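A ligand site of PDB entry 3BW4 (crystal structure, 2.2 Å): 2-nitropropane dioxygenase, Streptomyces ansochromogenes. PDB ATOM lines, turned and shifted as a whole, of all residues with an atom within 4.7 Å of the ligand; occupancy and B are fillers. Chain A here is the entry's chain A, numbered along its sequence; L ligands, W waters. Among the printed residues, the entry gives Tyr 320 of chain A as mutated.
N of Gly 216 sits at hydrogen-bond distance from O9 of the ligand (2.8 Å).
The backbone NH (N) of Thr 238 sits at hydrogen-bond distance from an oxygen (O7) of the ligand (3.0 Å).
O7 of the ligand sits at hydrogen-bond distance from OG1 of Thr 238 (2.8 Å).
N2 of the ligand sits at hydrogen-bond distance from OD1 of Asn 68.
An oxygen (O3) of the ligand is in hydrogen-bond range of the side-chain amide nitrogen of Gln 235 (3.0 Å).
The backbone NH (N) of Gly 237 sits at hydrogen-bond distance from an oxygen (O8) of the ligand.
The side-chain amide nitrogen (NE2) of Gln 172 sits at hydrogen-bond distance from an oxygen (O4) of the ligand.
An oxygen (O6) of the ligand is in hydrogen-bond range of the backbone NH (N) of Gly 177 (3.1 Å).
An oxygen (O2) of the ligand lies within hydrogen-bond range of the backbone NH of Ala 19, at 3.2 Å.
The backbone NH (N) of Gly 322 is in hydrogen-bond range of the side-chain hydroxyl (OG1) of Thr 238, 2.9 Å away.
The backbone carbonyl oxygen (O) of His 179 lies within hydrogen-bond range of the side-chain amide nitrogen (NE2) of Gln 172 (2.9 Å).
The backbone carbonyl oxygen (O) of Leu 236 is in hydrogen-bond range of the backbone NH (N) of Ala 16, at 2.9 Å.
The backbone carbonyl oxygen (O) of Tyr 320 lies within hydrogen-bond range of a ring nitrogen (NE2) of His 252, 3.0 Å away.
The backbone carbonyl oxygen (O) of Pro 17 sits close to a nitrogen (N3) of the ligand.
Ala 16 touches the ligand (CB to O3, 3.6 Å).
Met 18 touches the ligand (CA to N3, 3.2 Å).
Phe 70 touches the ligand (CZ to O2, 3.3 Å).
His 129 touches the ligand.
CA of Ala 176 touches O6 of the ligand (3.3 Å).
CA of Gly 178 touches C10 of the ligand (3.7 Å).
Ala 214 touches the ligand (CB to O4, 3.9 Å).
Gly 215 touches the ligand.
Leu 236 touches the ligand (CA to O8, 3.7 Å).
Leu 241 touches the ligand (CD2 to C7, 3.9 Å).
Tyr 320 touches the ligand (CB to C6, 3.6 Å).
Gly 322 touches the ligand.
Hydrophobic or aromatic side chains within 4 Å of the ligand: Ala 16, Pro 17, Met 18, Ala 19, Phe 70, His 129, Ala 176, Ala 214, Leu 241 and Tyr 320.
Within 4 Å of the ligand: Ala 16, Pro 17, Met 18, Ala 19, Asn 68, Phe 70, His 129, Gln 172, Ala 176, Gly 177, Gly 178, Ala 214, Gly 215, Gly 216, Gln 235, Leu 236, Gly 237, Thr 238, Leu 241, Tyr 320 and Gly 322.
The nearest printed residue that does not touch the ligand is Glu 175 (4.03 Å).
Water W5 lies within hydrogen-bond range of O8 of the ligand, O of Gln 235, N of Gly 215 and N of Ile 217.
Water W2 lies within hydrogen-bond range of the backbone carbonyl oxygen of Ile 217 (2.7 Å), an oxygen (O8) of the ligand (2.8 Å), the backbone NH of Gly 237 (3.2 Å) and the backbone NH of Thr 238 (3.4 Å).
Water W1 lies within hydrogen-bond range of an oxygen (O1) of the ligand and the side-chain amide nitrogen of Gln 235.
Water W4 lies within hydrogen-bond range of an oxygen (O2) of the ligand (2.9 Å) and the side-chain amide oxygen of Asn 68 (3.0 Å).
Water W3 bridges an oxygen (O9) of the ligand (3.0 Å) and the backbone carbonyl oxygen of Gly 322 (3.4 Å).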
ATOM      1  N   ALA A  16     -22.779 -34.247  12.876  1.00  0.00           N
ATOM      2  CA  ALA A  16     -22.792 -33.650  11.548  1.00  0.00           C
ATOM      3  C   ALA A  16     -21.416 -33.278  11.022  1.00  0.00           C
ATOM      4  O   ALA A  16     -20.558 -32.818  11.782  1.00  0.00           O
ATOM      5  CB  ALA A  16     -23.682 -32.412  11.545  1.00  0.00           C
ATOM      6  N   PRO A  17     -21.173 -33.494   9.729  1.00  0.00           N
ATOM      7  CA  PRO A  17     -19.862 -33.122   9.188  1.00  0.00           C
ATOM      8  C   PRO A  17     -19.862 -31.610   9.183  1.00  0.00           C
ATOM      9  O   PRO A  17     -20.888 -30.997   8.867  1.00  0.00           O
ATOM     10  CB  PRO A  17     -19.898 -33.709   7.771  1.00  0.00           C
ATOM     11  CG  PRO A  17     -21.355 -33.647   7.424  1.00  0.00           C
ATOM     12  CD  PRO A  17     -22.012 -34.128   8.706  1.00  0.00           C
ATOM     13  N   MET A  18     -18.749 -30.999   9.552  1.00  0.00           N
ATOM     14  CA  MET A  18     -18.672 -29.543   9.572  1.00  0.00           C
ATOM     15  C   MET A  18     -17.332 -29.120   8.986  1.00  0.00           C
ATOM     16  O   MET A  18     -16.280 -29.356   9.575  1.00  0.00           O
ATOM     17  CB  MET A  18     -18.845 -29.040  11.011  1.00  0.00           C
ATOM     18  CG  MET A  18     -20.199 -29.424  11.617  1.00  0.00           C
ATOM     19  SD  MET A  18     -20.486 -28.831  13.293  1.00  0.00           S
ATOM     20  CE  MET A  18     -19.878 -30.254  14.241  1.00  0.00           C
ATOM     21  N   ALA A  19     -17.397 -28.513   7.809  1.00  0.00           N
ATOM     22  CA  ALA A  19     -16.213 -28.064   7.095  1.00  0.00           C
ATOM     23  C   ALA A  19     -15.544 -26.894   7.807  1.00  0.00           C
ATOM     24  O   ALA A  19     -15.992 -26.468   8.871  1.00  0.00           O
ATOM     25  CB  ALA A  19     -16.587 -27.659   5.676  1.00  0.00           C
ATOM     26  N   VAL A  22     -13.651 -27.754  11.338  1.00  0.00           N
ATOM     27  CA  VAL A  22     -14.390 -28.005  12.564  1.00  0.00           C
ATOM     28  C   VAL A  22     -14.348 -29.465  12.976  1.00  0.00           C
ATOM     29  O   VAL A  22     -13.815 -29.808  14.031  1.00  0.00           O
ATOM     30  CB  VAL A  22     -15.868 -27.572  12.432  1.00  0.00           C
ATOM     31  CG1 VAL A  22     -16.644 -28.032  13.660  1.00  0.00           C
ATOM     32  CG2 VAL A  22     -15.948 -26.051  12.290  1.00  0.00           C
ATOM     33  N   ALA A  41     -15.554 -34.019   7.241  1.00  0.00           N
ATOM     34  CA  ALA A  41     -16.086 -33.115   6.237  1.00  0.00           C
ATOM     35  C   ALA A  41     -15.051 -32.951   5.118  1.00  0.00           C
ATOM     36  O   ALA A  41     -13.942 -32.501   5.370  1.00  0.00           O
ATOM     37  CB  ALA A  41     -16.377 -31.758   6.866  1.00  0.00           C
ATOM     38  N   ASN A  68     -18.539 -36.662   4.338  1.00  0.00           N
ATOM     39  CA  ASN A  68     -19.471 -35.825   3.593  1.00  0.00           C
ATOM     40  C   ASN A  68     -18.794 -35.088   2.433  1.00  0.00           C
ATOM     41  O   ASN A  68     -17.700 -34.547   2.580  1.00  0.00           O
ATOM     42  CB  ASN A  68     -20.128 -34.829   4.556  1.00  0.00           C
ATOM     43  CG  ASN A  68     -21.044 -33.831   3.859  1.00  0.00           C
ATOM     44  OD1 ASN A  68     -20.619 -32.741   3.496  1.00  0.00           O
ATOM     45  ND2 ASN A  68     -22.299 -34.225   3.676  1.00  0.00           N
ATOM     46  N   PHE A  70     -19.375 -32.309  -1.054  1.00  0.00           N
ATOM     47  CA  PHE A  70     -20.230 -31.302  -1.665  1.00  0.00           C
ATOM     48  C   PHE A  70     -20.487 -31.635  -3.134  1.00  0.00           C
ATOM     49  O   PHE A  70     -19.575 -32.049  -3.859  1.00  0.00           O
ATOM     50  CB  PHE A  70     -19.601 -29.908  -1.583  1.00  0.00           C
ATOM     51  CG  PHE A  70     -19.494 -29.363  -0.175  1.00  0.00           C
ATOM     52  CD1 PHE A  70     -20.178 -29.961   0.882  1.00  0.00           C
ATOM     53  CD2 PHE A  70     -18.748 -28.215   0.077  1.00  0.00           C
ATOM     54  CE1 PHE A  70     -20.124 -29.412   2.169  1.00  0.00           C
ATOM     55  CE2 PHE A  70     -18.678 -27.660   1.359  1.00  0.00           C
ATOM     56  CZ  PHE A  70     -19.364 -28.266   2.404  1.00  0.00           C
ATOM     57  N   HIS A 129     -24.066 -33.137   0.102  1.00  0.00           N
ATOM     58  CA  HIS A 129     -24.744 -31.886   0.413  1.00  0.00           C
ATOM     59  C   HIS A 129     -24.847 -31.003  -0.830  1.00  0.00           C
ATOM     60  O   HIS A 129     -23.980 -31.049  -1.703  1.00  0.00           O
ATOM     61  CB  HIS A 129     -23.990 -31.136   1.519  1.00  0.00           C
ATOM     62  CG  HIS A 129     -24.881 -30.357   2.441  1.00  0.00           C
ATOM     63  ND1 HIS A 129     -24.709 -29.008   2.691  1.00  0.00           N
ATOM     64  CD2 HIS A 129     -25.937 -30.740   3.198  1.00  0.00           C
ATOM     65  CE1 HIS A 129     -25.613 -28.606   3.565  1.00  0.00           C
ATOM     66  NE2 HIS A 129     -26.374 -29.642   3.890  1.00  0.00           N
ATOM     67  N   GLN A 172     -33.178 -31.803   6.855  1.00  0.00           N
ATOM     68  CA  GLN A 172     -32.593 -30.652   7.515  1.00  0.00           C
ATOM     69  C   GLN A 172     -33.590 -29.502   7.590  1.00  0.00           C
ATOM     70  O   GLN A 172     -33.947 -28.903   6.568  1.00  0.00           O
ATOM     71  CB  GLN A 172     -31.331 -30.203   6.764  1.00  0.00           C
ATOM     72  CG  GLN A 172     -30.627 -28.984   7.357  1.00  0.00           C
ATOM     73  CD  GLN A 172     -29.658 -28.334   6.378  1.00  0.00           C
ATOM     74  OE1 GLN A 172     -30.006 -28.100   5.222  1.00  0.00           O
ATOM     75  NE2 GLN A 172     -28.448 -28.032   6.852  1.00  0.00           N
ATOM     76  N   GLU A 175     -34.047 -24.539  11.235  1.00  0.00           N
ATOM     77  CA  GLU A 175     -33.281 -24.174  12.437  1.00  0.00           C
ATOM     78  C   GLU A 175     -31.807 -24.560  12.363  1.00  0.00           C
ATOM     79  O   GLU A 175     -30.985 -24.061  13.137  1.00  0.00           O
ATOM     80  CB  GLU A 175     -33.865 -24.845  13.686  1.00  0.00           C
ATOM     81  CG  GLU A 175     -35.375 -24.675  13.882  1.00  0.00           C
ATOM     82  CD  GLU A 175     -36.166 -25.820  13.289  1.00  0.00           C
ATOM     83  OE1 GLU A 175     -36.028 -26.070  12.066  1.00  0.00           O
ATOM     84  OE2 GLU A 175     -36.910 -26.467  14.033  1.00  0.00           O
ATOM     85  N   ALA A 176     -31.479 -25.475  11.462  1.00  0.00           N
ATOM     86  CA  ALA A 176     -30.114 -25.969  11.303  1.00  0.00           C
ATOM     87  C   ALA A 176     -29.058 -24.883  11.149  1.00  0.00           C
ATOM     88  O   ALA A 176     -29.323 -23.804  10.612  1.00  0.00           O
ATOM     89  CB  ALA A 176     -30.054 -26.934  10.109  1.00  0.00           C
ATOM     90  N   GLY A 177     -27.868 -25.170  11.657  1.00  0.00           N
ATOM     91  CA  GLY A 177     -26.761 -24.240  11.534  1.00  0.00           C
ATOM     92  C   GLY A 177     -26.044 -24.533  10.224  1.00  0.00           C
ATOM     93  O   GLY A 177     -26.257 -25.584   9.625  1.00  0.00           O
ATOM     94  N   GLY A 178     -25.205 -23.606   9.770  1.00  0.00           N
ATOM     95  CA  GLY A 178     -24.478 -23.817   8.533  1.00  0.00           C
ATOM     96  C   GLY A 178     -25.333 -23.715   7.286  1.00  0.00           C
ATOM     97  O   GLY A 178     -26.409 -23.108   7.301  1.00  0.00           O
ATOM     98  N   HIS A 179     -24.874 -24.316   6.196  1.00  0.00           N
ATOM     99  CA  HIS A 179     -25.586 -24.251   4.928  1.00  0.00           C
ATOM    100  C   HIS A 179     -26.848 -25.087   4.804  1.00  0.00           C
ATOM    101  O   HIS A 179     -26.890 -26.253   5.203  1.00  0.00           O
ATOM    102  CB  HIS A 179     -24.644 -24.593   3.767  1.00  0.00           C
ATOM    103  CG  HIS A 179     -23.733 -23.477   3.379  1.00  0.00           C
ATOM    104  ND1 HIS A 179     -22.595 -23.170   4.086  1.00  0.00           N
ATOM    105  CD2 HIS A 179     -23.823 -22.559   2.398  1.00  0.00           C
ATOM    106  CE1 HIS A 179     -22.027 -22.102   3.558  1.00  0.00           C
ATOM    107  NE2 HIS A 179     -22.747 -21.714   2.526  1.00  0.00           N
ATOM    108  N   ALA A 214     -32.270 -33.315  11.301  1.00  0.00           N
ATOM    109  CA  ALA A 214     -31.228 -32.327  11.587  1.00  0.00           C
ATOM    110  C   ALA A 214     -31.764 -30.902  11.720  1.00  0.00           C
ATOM    111  O   ALA A 214     -32.587 -30.444  10.919  1.00  0.00           O
ATOM    112  CB  ALA A 214     -30.170 -32.359  10.486  1.00  0.00           C
ATOM    113  N   GLY A 215     -31.277 -30.182  12.731  1.00  0.00           N
ATOM    114  CA  GLY A 215     -31.699 -28.810  12.923  1.00  0.00           C
ATOM    115  C   GLY A 215     -32.109 -28.419  14.331  1.00  0.00           C
ATOM    116  O   GLY A 215     -33.201 -28.760  14.772  1.00  0.00           O
ATOM    117  N   GLY A 216     -31.220 -27.704  15.028  1.00  0.00           N
ATOM    118  CA  GLY A 216     -31.511 -27.246  16.386  1.00  0.00           C
ATOM    119  C   GLY A 216     -31.511 -28.279  17.502  1.00  0.00           C
ATOM    120  O   GLY A 216     -31.926 -27.956  18.618  1.00  0.00           O
ATOM    121  N   ILE A 217     -31.056 -29.500  17.236  1.00  0.00           N
ATOM    122  CA  ILE A 217     -31.049 -30.526  18.272  1.00  0.00           C
ATOM    123  C   ILE A 217     -29.859 -30.364  19.213  1.00  0.00           C
ATOM    124  O   ILE A 217     -28.701 -30.544  18.820  1.00  0.00           O
ATOM    125  CB  ILE A 217     -31.053 -31.928  17.629  1.00  0.00           C
ATOM    126  CG1 ILE A 217     -32.267 -32.062  16.689  1.00  0.00           C
ATOM    127  CG2 ILE A 217     -31.097 -33.006  18.720  1.00  0.00           C
ATOM    128  CD1 ILE A 217     -32.346 -33.379  15.936  1.00  0.00           C
ATOM    129  N   GLN A 235     -29.153 -35.835  13.751  1.00  0.00           N
ATOM    130  CA  GLN A 235     -27.844 -35.337  13.366  1.00  0.00           C
ATOM    131  C   GLN A 235     -27.636 -33.968  14.027  1.00  0.00           C
ATOM    132  O   GLN A 235     -28.430 -33.046  13.838  1.00  0.00           O
ATOM    133  CB  GLN A 235     -27.732 -35.211  11.844  1.00  0.00           C
ATOM    134  CG  GLN A 235     -26.375 -34.676  11.379  1.00  0.00           C
ATOM    135  CD  GLN A 235     -26.106 -34.917   9.906  1.00  0.00           C
ATOM    136  OE1 GLN A 235     -26.101 -36.056   9.449  1.00  0.00           O
ATOM    137  NE2 GLN A 235     -25.888 -33.842   9.152  1.00  0.00           N
ATOM    138  N   LEU A 236     -26.554 -33.857  14.788  1.00  0.00           N
ATOM    139  CA  LEU A 236     -26.248 -32.630  15.515  1.00  0.00           C
ATOM    140  C   LEU A 236     -24.931 -32.006  15.084  1.00  0.00           C
ATOM    141  O   LEU A 236     -23.884 -32.654  15.092  1.00  0.00           O
ATOM    142  CB  LEU A 236     -26.165 -32.911  17.015  1.00  0.00           C
ATOM    143  CG  LEU A 236     -27.367 -33.467  17.782  1.00  0.00           C
ATOM    144  CD1 LEU A 236     -27.804 -34.802  17.208  1.00  0.00           C
ATOM    145  CD2 LEU A 236     -26.961 -33.622  19.242  1.00  0.00           C
ATOM    146  N   GLY A 237     -24.980 -30.718  14.740  1.00  0.00           N
ATOM    147  CA  GLY A 237     -23.785 -30.012  14.350  1.00  0.00           C
ATOM    148  C   GLY A 237     -23.342 -29.082  15.470  1.00  0.00           C
ATOM    149  O   GLY A 237     -22.333 -29.322  16.134  1.00  0.00           O
ATOM    150  N   THR A 238     -24.117 -28.033  15.686  1.00  0.00           N
ATOM    151  CA  THR A 238     -23.802 -27.037  16.708  1.00  0.00           C
ATOM    152  C   THR A 238     -23.484 -27.626  18.089  1.00  0.00           C
ATOM    153  O   THR A 238     -22.579 -27.137  18.774  1.00  0.00           O
ATOM    154  CB  THR A 238     -24.958 -26.014  16.826  1.00  0.00           C
ATOM    155  OG1 THR A 238     -25.177 -25.411  15.547  1.00  0.00           O
ATOM    156  CG2 THR A 238     -24.612 -24.924  17.834  1.00  0.00           C
ATOM    157  N   LEU A 241     -20.053 -28.656  17.868  1.00  0.00           N
ATOM    158  CA  LEU A 241     -19.161 -27.562  17.480  1.00  0.00           C
ATOM    159  C   LEU A 241     -18.434 -26.978  18.676  1.00  0.00           C
ATOM    160  O   LEU A 241     -17.287 -26.539  18.568  1.00  0.00           O
ATOM    161  CB  LEU A 241     -19.972 -26.460  16.786  1.00  0.00           C
ATOM    162  CG  LEU A 241     -19.239 -25.261  16.203  1.00  0.00           C
ATOM    163  CD1 LEU A 241     -18.168 -25.719  15.248  1.00  0.00           C
ATOM    164  CD2 LEU A 241     -20.218 -24.367  15.461  1.00  0.00           C
ATOM    165  N   HIS A 252     -15.228 -18.494  17.693  1.00  0.00           N
ATOM    166  CA  HIS A 252     -16.446 -19.113  17.209  1.00  0.00           C
ATOM    167  C   HIS A 252     -17.148 -19.865  18.340  1.00  0.00           C
ATOM    168  O   HIS A 252     -18.349 -19.698  18.554  1.00  0.00           O
ATOM    169  CB  HIS A 252     -16.114 -20.050  16.052  1.00  0.00           C
ATOM    170  CG  HIS A 252     -17.318 -20.512  15.275  1.00  0.00           C
ATOM    171  ND1 HIS A 252     -17.211 -21.088  14.024  1.00  0.00           N
ATOM    172  CD2 HIS A 252     -18.629 -20.495  15.582  1.00  0.00           C
ATOM    173  CE1 HIS A 252     -18.422 -21.399  13.590  1.00  0.00           C
ATOM    174  NE2 HIS A 252     -19.297 -21.051  14.519  1.00  0.00           N
ATOM    175  N   TYR A 320     -21.222 -19.970  11.820  1.00  0.00           N
ATOM    176  CA  TYR A 320     -22.313 -20.919  11.566  1.00  0.00           C
ATOM    177  C   TYR A 320     -22.818 -21.520  12.886  1.00  0.00           C
ATOM    178  O   TYR A 320     -22.031 -21.940  13.736  1.00  0.00           O
ATOM    179  CB  TYR A 320     -21.836 -22.042  10.640  1.00  0.00           C
ATOM    180  CG  TYR A 320     -21.332 -21.560   9.302  1.00  0.00           C
ATOM    181  CD1 TYR A 320     -20.088 -21.968   8.821  1.00  0.00           C
ATOM    182  CD2 TYR A 320     -22.092 -20.683   8.533  1.00  0.00           C
ATOM    183  CE1 TYR A 320     -19.605 -21.500   7.605  1.00  0.00           C
ATOM    184  CE2 TYR A 320     -21.622 -20.213   7.317  1.00  0.00           C
ATOM    185  CZ  TYR A 320     -20.378 -20.622   6.853  1.00  0.00           C
ATOM    186  OH  TYR A 320     -19.901 -20.113   5.679  1.00  0.00           O
ATOM    187  N   ALA A 321     -24.141 -21.544  13.052  1.00  0.00           N
ATOM    188  CA  ALA A 321     -24.735 -22.067  14.268  1.00  0.00           C
ATOM    189  C   ALA A 321     -26.257 -22.189  14.103  1.00  0.00           C
ATOM    190  O   ALA A 321     -26.874 -21.371  13.426  1.00  0.00           O
ATOM    191  CB  ALA A 321     -24.409 -21.151  15.447  1.00  0.00           C
ATOM    192  N   GLY A 322     -26.823 -23.224  14.720  1.00  0.00           N
ATOM    193  CA  GLY A 322     -28.261 -23.448  14.641  1.00  0.00           C
ATOM    194  C   GLY A 322     -28.967 -22.617  15.690  1.00  0.00           C
ATOM    195  O   GLY A 322     -28.333 -22.025  16.558  1.00  0.00           O
HETATM  196  N1  LIG L   1     -23.456 -30.106   6.511  1.00  0.00           N
HETATM  197  C1  LIG L   1     -22.807 -30.778   5.471  1.00  0.00           C
HETATM  198  O1  LIG L   1     -23.410 -31.635   4.832  1.00  0.00           O
HETATM  199  N2  LIG L   1     -21.485 -30.497   5.162  1.00  0.00           N
HETATM  200  C2  LIG L   1     -20.741 -29.548   5.850  1.00  0.00           C
HETATM  201  O2  LIG L   1     -19.559 -29.325   5.546  1.00  0.00           O
HETATM  202  C3  LIG L   1     -21.385 -28.853   6.908  1.00  0.00           C
HETATM  203  N3  LIG L   1     -20.696 -27.897   7.666  1.00  0.00           N
HETATM  204  C4  LIG L   1     -21.297 -27.239   8.733  1.00  0.00           C
HETATM  205  C5  LIG L   1     -20.544 -26.290   9.479  1.00  0.00           C
HETATM  206  C6  LIG L   1     -21.104 -25.576  10.606  1.00  0.00           C
HETATM  207  C7  LIG L   1     -20.079 -25.279  11.713  1.00  0.00           C
HETATM  208  C8  LIG L   1     -22.468 -25.933  10.935  1.00  0.00           C
HETATM  209  C9  LIG L   1     -23.013 -25.893  12.363  1.00  0.00           C
HETATM  210  C10 LIG L   1     -23.246 -26.861  10.180  1.00  0.00           C
HETATM  211  C11 LIG L   1     -22.661 -27.521   9.067  1.00  0.00           C
HETATM  212  N4  LIG L   1     -23.379 -28.472   8.291  1.00  0.00           N
HETATM  213  C12 LIG L   1     -22.753 -29.151   7.235  1.00  0.00           C
HETATM  214  C13 LIG L   1     -24.894 -28.649   8.488  1.00  0.00           C
HETATM  215  C14 LIG L   1     -25.101 -29.923   9.347  1.00  0.00           C
HETATM  216  O3  LIG L   1     -25.085 -31.058   8.509  1.00  0.00           O
HETATM  217  C15 LIG L   1     -26.484 -29.927  10.105  1.00  0.00           C
HETATM  218  O4  LIG L   1     -27.496 -29.812   9.116  1.00  0.00           O
HETATM  219  C16 LIG L   1     -26.666 -28.778  11.108  1.00  0.00           C
HETATM  220  O5  LIG L   1     -25.480 -28.652  11.880  1.00  0.00           O
HETATM  221  C17 LIG L   1     -27.867 -29.072  12.039  1.00  0.00           C
HETATM  222  O6  LIG L   1     -28.087 -28.009  12.993  1.00  0.00           O
HETATM  223  P1  LIG L   1     -27.394 -27.806  14.465  1.00  0.00           P
HETATM  224  O7  LIG L   1     -26.249 -27.210  13.706  1.00  0.00           O
HETATM  225  O8  LIG L   1     -27.628 -29.282  14.597  1.00  0.00           O
HETATM  226  O9  LIG L   1     -28.588 -26.893  14.699  1.00  0.00           O
HETATM  227  O   HOH W   1     -25.121 -33.507   6.224  1.00  0.00           O
HETATM  228  O   HOH W   2     -26.691 -29.652  17.251  1.00  0.00           O
HETATM  229  O   HOH W   3     -28.624 -25.357  17.246  1.00  0.00           O
HETATM  230  O   HOH W   4     -18.015 -31.356   4.139  1.00  0.00           O
HETATM  231  O   HOH W   5     -29.505 -30.883  14.937  1.00  0.00           O
HETATM  232  O   HOH W   6     -27.499 -31.603   6.835  1.00  0.00           O
